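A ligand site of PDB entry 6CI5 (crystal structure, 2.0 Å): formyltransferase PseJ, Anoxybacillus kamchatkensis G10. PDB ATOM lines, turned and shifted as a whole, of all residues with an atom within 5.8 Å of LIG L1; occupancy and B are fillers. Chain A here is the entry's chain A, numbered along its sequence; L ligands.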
ATOM      1  N   SER A  71     -25.332 -24.780  29.934  1.00  0.00           N
ATOM      2  CA  SER A  71     -25.263 -23.810  28.851  1.00  0.00           C
ATOM      3  C   SER A  71     -25.217 -24.555  27.518  1.00  0.00           C
ATOM      4  O   SER A  71     -24.357 -25.422  27.318  1.00  0.00           O
ATOM      5  CB  SER A  71     -24.040 -22.915  28.995  1.00  0.00           C
ATOM      6  OG  SER A  71     -23.977 -21.970  27.937  1.00  0.00           O
ATOM      7  N   TYR A  74     -26.069 -20.684  24.544  1.00  0.00           N
ATOM      8  CA  TYR A  74     -26.132 -19.404  25.218  1.00  0.00           C
ATOM      9  C   TYR A  74     -25.173 -18.416  24.548  1.00  0.00           C
ATOM     10  O   TYR A  74     -24.005 -18.739  24.307  1.00  0.00           O
ATOM     11  CB  TYR A  74     -25.793 -19.572  26.696  1.00  0.00           C
ATOM     12  CG  TYR A  74     -26.052 -18.339  27.532  1.00  0.00           C
ATOM     13  CD1 TYR A  74     -27.295 -17.722  27.532  1.00  0.00           C
ATOM     14  CD2 TYR A  74     -25.051 -17.798  28.335  1.00  0.00           C
ATOM     15  CE1 TYR A  74     -27.540 -16.596  28.296  1.00  0.00           C
ATOM     16  CE2 TYR A  74     -25.287 -16.682  29.100  1.00  0.00           C
ATOM     17  CZ  TYR A  74     -26.525 -16.080  29.076  1.00  0.00           C
ATOM     18  OH  TYR A  74     -26.760 -14.965  29.841  1.00  0.00           O
ATOM     19  N   ARG A  75     -25.666 -17.218  24.256  1.00  0.00           N
ATOM     20  CA  ARG A  75     -24.948 -16.262  23.426  1.00  0.00           C
ATOM     21  C   ARG A  75     -24.361 -15.106  24.245  1.00  0.00           C
ATOM     22  O   ARG A  75     -24.240 -13.989  23.741  1.00  0.00           O
ATOM     23  CB  ARG A  75     -25.872 -15.713  22.345  1.00  0.00           C
ATOM     24  CG  ARG A  75     -26.607 -16.795  21.557  1.00  0.00           C
ATOM     25  CD  ARG A  75     -27.195 -16.252  20.274  1.00  0.00           C
ATOM     26  NE  ARG A  75     -26.165 -15.774  19.357  1.00  0.00           N
ATOM     27  CZ  ARG A  75     -25.413 -16.556  18.591  1.00  0.00           C
ATOM     28  NH1 ARG A  75     -24.502 -16.022  17.794  1.00  0.00           N
ATOM     29  NH2 ARG A  75     -25.562 -17.872  18.625  1.00  0.00           N
ATOM     30  N   TYR A  76     -23.991 -15.359  25.493  1.00  0.00           N
ATOM     31  CA  TYR A  76     -23.395 -14.341  26.338  1.00  0.00           C
ATOM     32  C   TYR A  76     -22.361 -14.976  27.249  1.00  0.00           C
ATOM     33  O   TYR A  76     -22.445 -16.151  27.592  1.00  0.00           O
ATOM     34  CB  TYR A  76     -24.446 -13.611  27.187  1.00  0.00           C
ATOM     35  CG  TYR A  76     -25.579 -13.010  26.380  1.00  0.00           C
ATOM     36  CD1 TYR A  76     -25.411 -11.783  25.743  1.00  0.00           C
ATOM     37  CD2 TYR A  76     -26.800 -13.646  26.270  1.00  0.00           C
ATOM     38  CE1 TYR A  76     -26.438 -11.225  25.006  1.00  0.00           C
ATOM     39  CE2 TYR A  76     -27.830 -13.100  25.540  1.00  0.00           C
ATOM     40  CZ  TYR A  76     -27.652 -11.884  24.904  1.00  0.00           C
ATOM     41  OH  TYR A  76     -28.672 -11.338  24.177  1.00  0.00           O
ATOM     42  N   ILE A  77     -21.373 -14.174  27.631  1.00  0.00           N
ATOM     43  CA  ILE A  77     -20.335 -14.617  28.552  1.00  0.00           C
ATOM     44  C   ILE A  77     -20.890 -14.589  29.966  1.00  0.00           C
ATOM     45  O   ILE A  77     -21.561 -13.631  30.379  1.00  0.00           O
ATOM     46  CB  ILE A  77     -19.079 -13.728  28.430  1.00  0.00           C
ATOM     47  CG1 ILE A  77     -18.539 -13.770  26.988  1.00  0.00           C
ATOM     48  CG2 ILE A  77     -18.001 -14.180  29.401  1.00  0.00           C
ATOM     49  CD1 ILE A  77     -17.521 -12.695  26.688  1.00  0.00           C
ATOM     50  N   ILE A  78     -20.615 -15.649  30.716  1.00  0.00           N
ATOM     51  CA  ILE A  78     -21.083 -15.775  32.088  1.00  0.00           C
ATOM     52  C   ILE A  78     -20.084 -15.094  33.004  1.00  0.00           C
ATOM     53  O   ILE A  78     -18.866 -15.334  32.909  1.00  0.00           O
ATOM     54  CB  ILE A  78     -21.279 -17.255  32.465  1.00  0.00           C
ATOM     55  CG1 ILE A  78     -22.347 -17.875  31.544  1.00  0.00           C
ATOM     56  CG2 ILE A  78     -21.688 -17.399  33.931  1.00  0.00           C
ATOM     57  CD1 ILE A  78     -22.471 -19.381  31.660  1.00  0.00           C
ATOM     58  N   HIS A  79     -20.577 -14.244  33.901  1.00  0.00           N
ATOM     59  CA  HIS A  79     -19.702 -13.410  34.714  1.00  0.00           C
ATOM     60  C   HIS A  79     -18.786 -14.289  35.566  1.00  0.00           C
ATOM     61  O   HIS A  79     -19.201 -15.367  36.015  1.00  0.00           O
ATOM     62  CB  HIS A  79     -20.533 -12.493  35.614  1.00  0.00           C
ATOM     63  CG  HIS A  79     -19.768 -11.313  36.125  1.00  0.00           C
ATOM     64  ND1 HIS A  79     -18.969 -11.371  37.247  1.00  0.00           N
ATOM     65  CD2 HIS A  79     -19.673 -10.043  35.668  1.00  0.00           C
ATOM     66  CE1 HIS A  79     -18.422 -10.183  37.463  1.00  0.00           C
ATOM     67  NE2 HIS A  79     -18.833  -9.359  36.514  1.00  0.00           N
ATOM     68  N   VAL A  83     -19.386 -17.843  37.605  1.00  0.00           N
ATOM     69  CA  VAL A  83     -18.503 -18.984  37.353  1.00  0.00           C
ATOM     70  C   VAL A  83     -18.010 -19.568  38.678  1.00  0.00           C
ATOM     71  O   VAL A  83     -18.157 -20.767  38.937  1.00  0.00           O
ATOM     72  CB  VAL A  83     -17.327 -18.551  36.464  1.00  0.00           C
ATOM     73  CG1 VAL A  83     -16.248 -19.633  36.431  1.00  0.00           C
ATOM     74  CG2 VAL A  83     -17.820 -18.254  35.047  1.00  0.00           C
ATOM     75  N   ASN A  92     -20.962 -26.504  29.899  1.00  0.00           N
ATOM     76  CA  ASN A  92     -21.342 -25.936  28.610  1.00  0.00           C
ATOM     77  C   ASN A  92     -21.220 -27.022  27.550  1.00  0.00           C
ATOM     78  O   ASN A  92     -20.235 -27.772  27.532  1.00  0.00           O
ATOM     79  CB  ASN A  92     -20.450 -24.737  28.252  1.00  0.00           C
ATOM     80  CG  ASN A  92     -20.791 -24.154  26.891  1.00  0.00           C
ATOM     81  OD1 ASN A  92     -21.886 -23.616  26.691  1.00  0.00           O
ATOM     82  ND2 ASN A  92     -19.851 -24.246  25.959  1.00  0.00           N
ATOM     83  N   HIS A  94     -20.449 -27.587  23.954  1.00  0.00           N
ATOM     84  CA  HIS A  94     -19.738 -26.861  22.905  1.00  0.00           C
ATOM     85  C   HIS A  94     -19.502 -27.811  21.734  1.00  0.00           C
ATOM     86  O   HIS A  94     -18.895 -28.872  21.914  1.00  0.00           O
ATOM     87  CB  HIS A  94     -18.422 -26.298  23.423  1.00  0.00           C
ATOM     88  CG  HIS A  94     -17.737 -25.368  22.473  1.00  0.00           C
ATOM     89  ND1 HIS A  94     -18.289 -24.161  22.085  1.00  0.00           N
ATOM     90  CD2 HIS A  94     -16.548 -25.456  21.835  1.00  0.00           C
ATOM     91  CE1 HIS A  94     -17.467 -23.557  21.238  1.00  0.00           C
ATOM     92  NE2 HIS A  94     -16.406 -24.327  21.076  1.00  0.00           N
ATOM     93  N   HIS A 122     -17.814 -29.512  28.840  1.00  0.00           N
ATOM     94  CA  HIS A 122     -16.749 -29.025  29.711  1.00  0.00           C
ATOM     95  C   HIS A 122     -17.339 -28.154  30.798  1.00  0.00           C
ATOM     96  O   HIS A 122     -18.344 -27.460  30.590  1.00  0.00           O
ATOM     97  CB  HIS A 122     -15.696 -28.235  28.918  1.00  0.00           C
ATOM     98  CG  HIS A 122     -16.197 -26.934  28.373  1.00  0.00           C
ATOM     99  ND1 HIS A 122     -16.130 -25.754  29.089  1.00  0.00           N
ATOM    100  CD2 HIS A 122     -16.788 -26.627  27.197  1.00  0.00           C
ATOM    101  CE1 HIS A 122     -16.641 -24.774  28.368  1.00  0.00           C
ATOM    102  NE2 HIS A 122     -17.051 -25.276  27.215  1.00  0.00           N
ATOM    103  N   TYR A 123     -16.705 -28.194  31.967  1.00  0.00           N
ATOM    104  CA  TYR A 123     -17.060 -27.274  33.029  1.00  0.00           C
ATOM    105  C   TYR A 123     -16.805 -25.839  32.573  1.00  0.00           C
ATOM    106  O   TYR A 123     -15.881 -25.557  31.810  1.00  0.00           O
ATOM    107  CB  TYR A 123     -16.265 -27.577  34.298  1.00  0.00           C
ATOM    108  CG  TYR A 123     -16.720 -28.824  35.017  1.00  0.00           C
ATOM    109  CD1 TYR A 123     -17.932 -28.855  35.688  1.00  0.00           C
ATOM    110  CD2 TYR A 123     -15.923 -29.962  35.039  1.00  0.00           C
ATOM    111  CE1 TYR A 123     -18.350 -29.989  36.356  1.00  0.00           C
ATOM    112  CE2 TYR A 123     -16.341 -31.105  35.705  1.00  0.00           C
ATOM    113  CZ  TYR A 123     -17.549 -31.113  36.361  1.00  0.00           C
ATOM    114  OH  TYR A 123     -17.967 -32.247  37.029  1.00  0.00           O
ATOM    115  N   ILE A 124     -17.647 -24.936  33.047  1.00  0.00           N
ATOM    116  CA  ILE A 124     -17.544 -23.517  32.708  1.00  0.00           C
ATOM    117  C   ILE A 124     -16.579 -22.866  33.673  1.00  0.00           C
ATOM    118  O   ILE A 124     -16.673 -23.048  34.894  1.00  0.00           O
ATOM    119  CB  ILE A 124     -18.931 -22.840  32.759  1.00  0.00           C
ATOM    120  CG1 ILE A 124     -19.816 -23.398  31.644  1.00  0.00           C
ATOM    121  CG2 ILE A 124     -18.792 -21.321  32.628  1.00  0.00           C
ATOM    122  CD1 ILE A 124     -21.259 -22.904  31.685  1.00  0.00           C
ATOM    123  N   ASP A 125     -15.629 -22.100  33.133  1.00  0.00           N
ATOM    124  CA  ASP A 125     -14.688 -21.330  33.917  1.00  0.00           C
ATOM    125  C   ASP A 125     -14.610 -19.923  33.338  1.00  0.00           C
ATOM    126  O   ASP A 125     -15.215 -19.625  32.304  1.00  0.00           O
ATOM    127  CB  ASP A 125     -13.301 -21.984  33.956  1.00  0.00           C
ATOM    128  CG  ASP A 125     -12.606 -21.953  32.610  1.00  0.00           C
ATOM    129  OD1 ASP A 125     -13.255 -21.619  31.594  1.00  0.00           O
ATOM    130  OD2 ASP A 125     -11.392 -22.255  32.564  1.00  0.00           O
ATOM    131  N   SER A 126     -13.852 -19.050  34.003  1.00  0.00           N
ATOM    132  CA  SER A 126     -13.565 -17.744  33.434  1.00  0.00           C
ATOM    133  C   SER A 126     -12.850 -17.929  32.100  1.00  0.00           C
ATOM    134  O   SER A 126     -11.992 -18.797  31.952  1.00  0.00           O
ATOM    135  CB  SER A 126     -12.716 -16.921  34.395  1.00  0.00           C
ATOM    136  OG  SER A 126     -11.509 -17.594  34.711  1.00  0.00           O
ATOM    137  N   GLY A 127     -13.214 -17.111  31.130  1.00  0.00           N
ATOM    138  CA  GLY A 127     -12.703 -17.306  29.786  1.00  0.00           C
ATOM    139  C   GLY A 127     -13.607 -18.198  28.954  1.00  0.00           C
ATOM    140  O   GLY A 127     -14.328 -19.049  29.470  1.00  0.00           O
ATOM    141  N   LEU A 128     -13.552 -17.998  27.643  1.00  0.00           N
ATOM    142  CA  LEU A 128     -14.508 -18.598  26.733  1.00  0.00           C
ATOM    143  C   LEU A 128     -14.042 -19.991  26.336  1.00  0.00           C
ATOM    144  O   LEU A 128     -13.082 -20.148  25.573  1.00  0.00           O
ATOM    145  CB  LEU A 128     -14.695 -17.704  25.507  1.00  0.00           C
ATOM    146  CG  LEU A 128     -15.857 -18.003  24.557  1.00  0.00           C
ATOM    147  CD1 LEU A 128     -17.164 -18.164  25.304  1.00  0.00           C
ATOM    148  CD2 LEU A 128     -16.000 -16.893  23.525  1.00  0.00           C
ATOM    149  N   ASP A 129     -14.722 -21.018  26.867  1.00  0.00           N
ATOM    150  CA  ASP A 129     -14.528 -22.409  26.444  1.00  0.00           C
ATOM    151  C   ASP A 129     -13.144 -22.928  26.815  1.00  0.00           C
ATOM    152  O   ASP A 129     -12.525 -23.672  26.056  1.00  0.00           O
ATOM    153  CB  ASP A 129     -14.767 -22.560  24.934  1.00  0.00           C
ATOM    154  CG  ASP A 129     -16.129 -22.061  24.512  1.00  0.00           C
ATOM    155  OD1 ASP A 129     -17.087 -22.207  25.306  1.00  0.00           O
ATOM    156  OD2 ASP A 129     -16.251 -21.524  23.385  1.00  0.00           O
ATOM    157  N   THR A 130     -12.663 -22.554  28.001  1.00  0.00           N
ATOM    158  CA  THR A 130     -11.353 -22.973  28.480  1.00  0.00           C
ATOM    159  C   THR A 130     -11.404 -23.861  29.711  1.00  0.00           C
ATOM    160  O   THR A 130     -10.354 -24.196  30.259  1.00  0.00           O
ATOM    161  CB  THR A 130     -10.476 -21.749  28.786  1.00  0.00           C
ATOM    162  OG1 THR A 130     -11.173 -20.870  29.681  1.00  0.00           O
ATOM    163  CG2 THR A 130     -10.103 -21.003  27.521  1.00  0.00           C
ATOM    164  N   GLY A 131     -12.599 -24.258  30.173  1.00  0.00           N
ATOM    165  CA  GLY A 131     -12.712 -25.029  31.381  1.00  0.00           C
ATOM    166  C   GLY A 131     -12.332 -26.489  31.201  1.00  0.00           C
ATOM    167  O   GLY A 131     -12.075 -26.973  30.101  1.00  0.00           O
HETATM  168  N1  LIG L   1     -17.276 -19.758  29.852  1.00  0.00           N
HETATM  169  C1  LIG L   1     -18.087 -18.524  30.204  1.00  0.00           C
HETATM  170  N2  LIG L   1     -19.396 -18.267  29.523  1.00  0.00           N
HETATM  171  C2  LIG L   1     -19.899 -19.209  28.517  1.00  0.00           C
HETATM  172  C3  LIG L   1     -19.088 -20.453  28.163  1.00  0.00           C
HETATM  173  C4  LIG L   1     -17.771 -20.703  28.858  1.00  0.00           C
HETATM  174  N3  LIG L   1     -21.091 -18.936  27.911  1.00  0.00           N
HETATM  175  C5  LIG L   1     -21.586 -19.990  26.853  1.00  0.00           C
HETATM  176  C6  LIG L   1     -20.601 -20.738  26.235  1.00  0.00           C
HETATM  177  N4  LIG L   1     -19.536 -21.340  27.235  1.00  0.00           N
HETATM  178  C7  LIG L   1     -19.899 -19.873  25.203  1.00  0.00           C
HETATM  179  O1  LIG L   1     -17.136 -21.671  28.592  1.00  0.00           O
HETATM  180  N5  LIG L   1     -17.591 -17.589  31.196  1.00  0.00           N
HETATM  181  C1  LG2 L   2     -27.985 -21.233  14.229  1.00  0.00           C
HETATM  182  C2  LG2 L   2     -28.371 -23.401  13.531  1.00  0.00           C
HETATM  183  C3  LG2 L   2     -25.686 -24.594  10.225  1.00  0.00           C
HETATM  184  C4  LG2 L   2     -23.706 -22.923  11.749  1.00  0.00           C
HETATM  185  C5  LG2 L   2     -21.175 -20.983  21.006  1.00  0.00           C
HETATM  186  C6  LG2 L   2     -20.632 -22.423  23.067  1.00  0.00           C
HETATM  187  C7  LG2 L   2     -21.753 -22.243  20.346  1.00  0.00           C
HETATM  188  C8  LG2 L   2     -20.644 -23.105  19.841  1.00  0.00           C
HETATM  189  C9  LG2 L   2     -23.737 -20.996  19.674  1.00  0.00           C
HETATM  190  C10 LG2 L   2     -28.537 -22.165  13.171  1.00  0.00           C
HETATM  191  C11 LG2 L   2     -28.237 -24.150  12.219  1.00  0.00           C
HETATM  192  C12 LG2 L   2     -27.557 -23.135  11.255  1.00  0.00           C
HETATM  193  C13 LG2 L   2     -23.243 -24.008  10.901  1.00  0.00           C
HETATM  194  C14 LG2 L   2     -25.130 -22.646  11.854  1.00  0.00           C
HETATM  195  C15 LG2 L   2     -23.196 -19.741  20.355  1.00  0.00           C
HETATM  196  C16 LG2 L   2     -22.252 -17.512  19.511  1.00  0.00           C
HETATM  197  C17 LG2 L   2     -22.788 -16.792  20.738  1.00  0.00           C
HETATM  198  C18 LG2 L   2     -22.272 -20.082  21.469  1.00  0.00           C
HETATM  199  N1  LG2 L   2     -20.290 -21.350  22.147  1.00  0.00           N
HETATM  200  N2  LG2 L   2     -26.107 -23.448  11.128  1.00  0.00           N
HETATM  201  N3  LG2 L   2     -24.176 -24.827  10.161  1.00  0.00           N
HETATM  202  N4  LG2 L   2     -22.450 -18.940  19.341  1.00  0.00           N
HETATM  203  O1  LG2 L   2     -19.900 -22.690  23.960  1.00  0.00           O
HETATM  204  O2  LG2 L   2     -22.652 -21.889  19.219  1.00  0.00           O
HETATM  205  O3  LG2 L   2     -24.491 -20.657  18.580  1.00  0.00           O
HETATM  206  O4  LG2 L   2     -26.538 -22.132  19.120  1.00  0.00           O
HETATM  207  O5  LG2 L   2     -26.379 -21.195  16.717  1.00  0.00           O
HETATM  208  O6  LG2 L   2     -26.599 -21.146  14.044  1.00  0.00           O
HETATM  209  O7  LG2 L   2     -22.079 -24.221  10.819  1.00  0.00           O
HETATM  210  O8  LG2 L   2     -26.463 -25.257   9.630  1.00  0.00           O
HETATM  211  O9  LG2 L   2     -27.713 -21.980  11.784  1.00  0.00           O
HETATM  212  O10 LG2 L   2     -29.464 -24.507  11.745  1.00  0.00           O
HETATM  213  O11 LG2 L   2     -29.571 -23.911  14.294  1.00  0.00           O
HETATM  214  O12 LG2 L   2     -24.292 -21.385  15.196  1.00  0.00           O
HETATM  215  O13 LG2 L   2     -25.458 -19.222  15.329  1.00  0.00           O
HETATM  216  O14 LG2 L   2     -24.802 -23.027  17.627  1.00  0.00           O
HETATM  217  O15 LG2 L   2     -21.660 -16.904  18.681  1.00  0.00           O
HETATM  218  O16 LG2 L   2     -23.022 -20.767  22.517  1.00  0.00           O
HETATM  219  P1  LG2 L   2     -25.562 -21.782  18.026  1.00  0.00           P
HETATM  220  P2  LG2 L   2     -25.647 -20.715  15.327  1.00  0.00           P
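N of Gly 131 lies within hydrogen-bond range of OD1 of Asp 125, 3.1 Å away. The side-chain amide nitrogen (ND2) of Asn 92 sits at hydrogen-bond distance from the side-chain carboxylate (OD1) of Asp 129. OD1 of Asp 125 lies within hydrogen-bond range of OG1 of Thr 130. The backbone NH (N) of Asn 92 lies within hydrogen-bond range of the backbone carbonyl oxygen (O) of His 122 (2.9 Å). The side-chain hydroxyl (OG) of Ser 71 is in hydrogen-bond range of the side-chain amide oxygen (OD1) of Asn 92.
Merely in contact with LIG L1: His 122 (3.2 Å), Leu 128 (3.2 Å), Ser 71 (3.3 Å), Ile 124 (3.5 Å), Tyr 74 (3.7 Å), Ile 77 (3.9 Å) and Val 83 (3.9 Å). Hydrophobic or aromatic side chains within 4 Å of LIG L1: Ile 77, Ile 78, Val 83, His 122, Ile 124 and Leu 128. The nearest printed residue that does not touch LIG L1 is Thr 130 (4.6 Å).
The backbone carbonyl oxygen of Tyr 74 lies within hydrogen-bond range of an oxygen (O16) of LG2 L2 (2.9 Å). The backbone carbonyl oxygen (O) of Tyr 76 lies within hydrogen-bond range of a nitrogen (N3) of LIG L1, 3.1 Å away. N1 of LIG L1 sits at hydrogen-bond distance from O of Gly 127, 3.1 Å away. ND1 of His 94 is in hydrogen-bond range of O1 of LG2 L2 (2.9 Å). ND2 of Asn 92 is in hydrogen-bond range of O1 of LG2 L2, 2.5 Å away. NH2 of Arg 75 lies within salt-bridge range of O13 of LG2 L2. N2 of LIG L1 sits at hydrogen-bond distance from N of Ile 78. N of Asp 129 sits at hydrogen-bond distance from O1 of LIG L1 (3.0 Å). N5 of LIG L1 is in hydrogen-bond range of O of Ile 78. A nitrogen (N1) of LIG L1 lies within hydrogen-bond range of the backbone carbonyl oxygen (O) of Asp 125. N4 of LIG L1 sits close to ND2 of Asn 92 (3.2 Å). OD1 of Asp 129 is in hydrogen-bond range of N4 of LIG L1.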
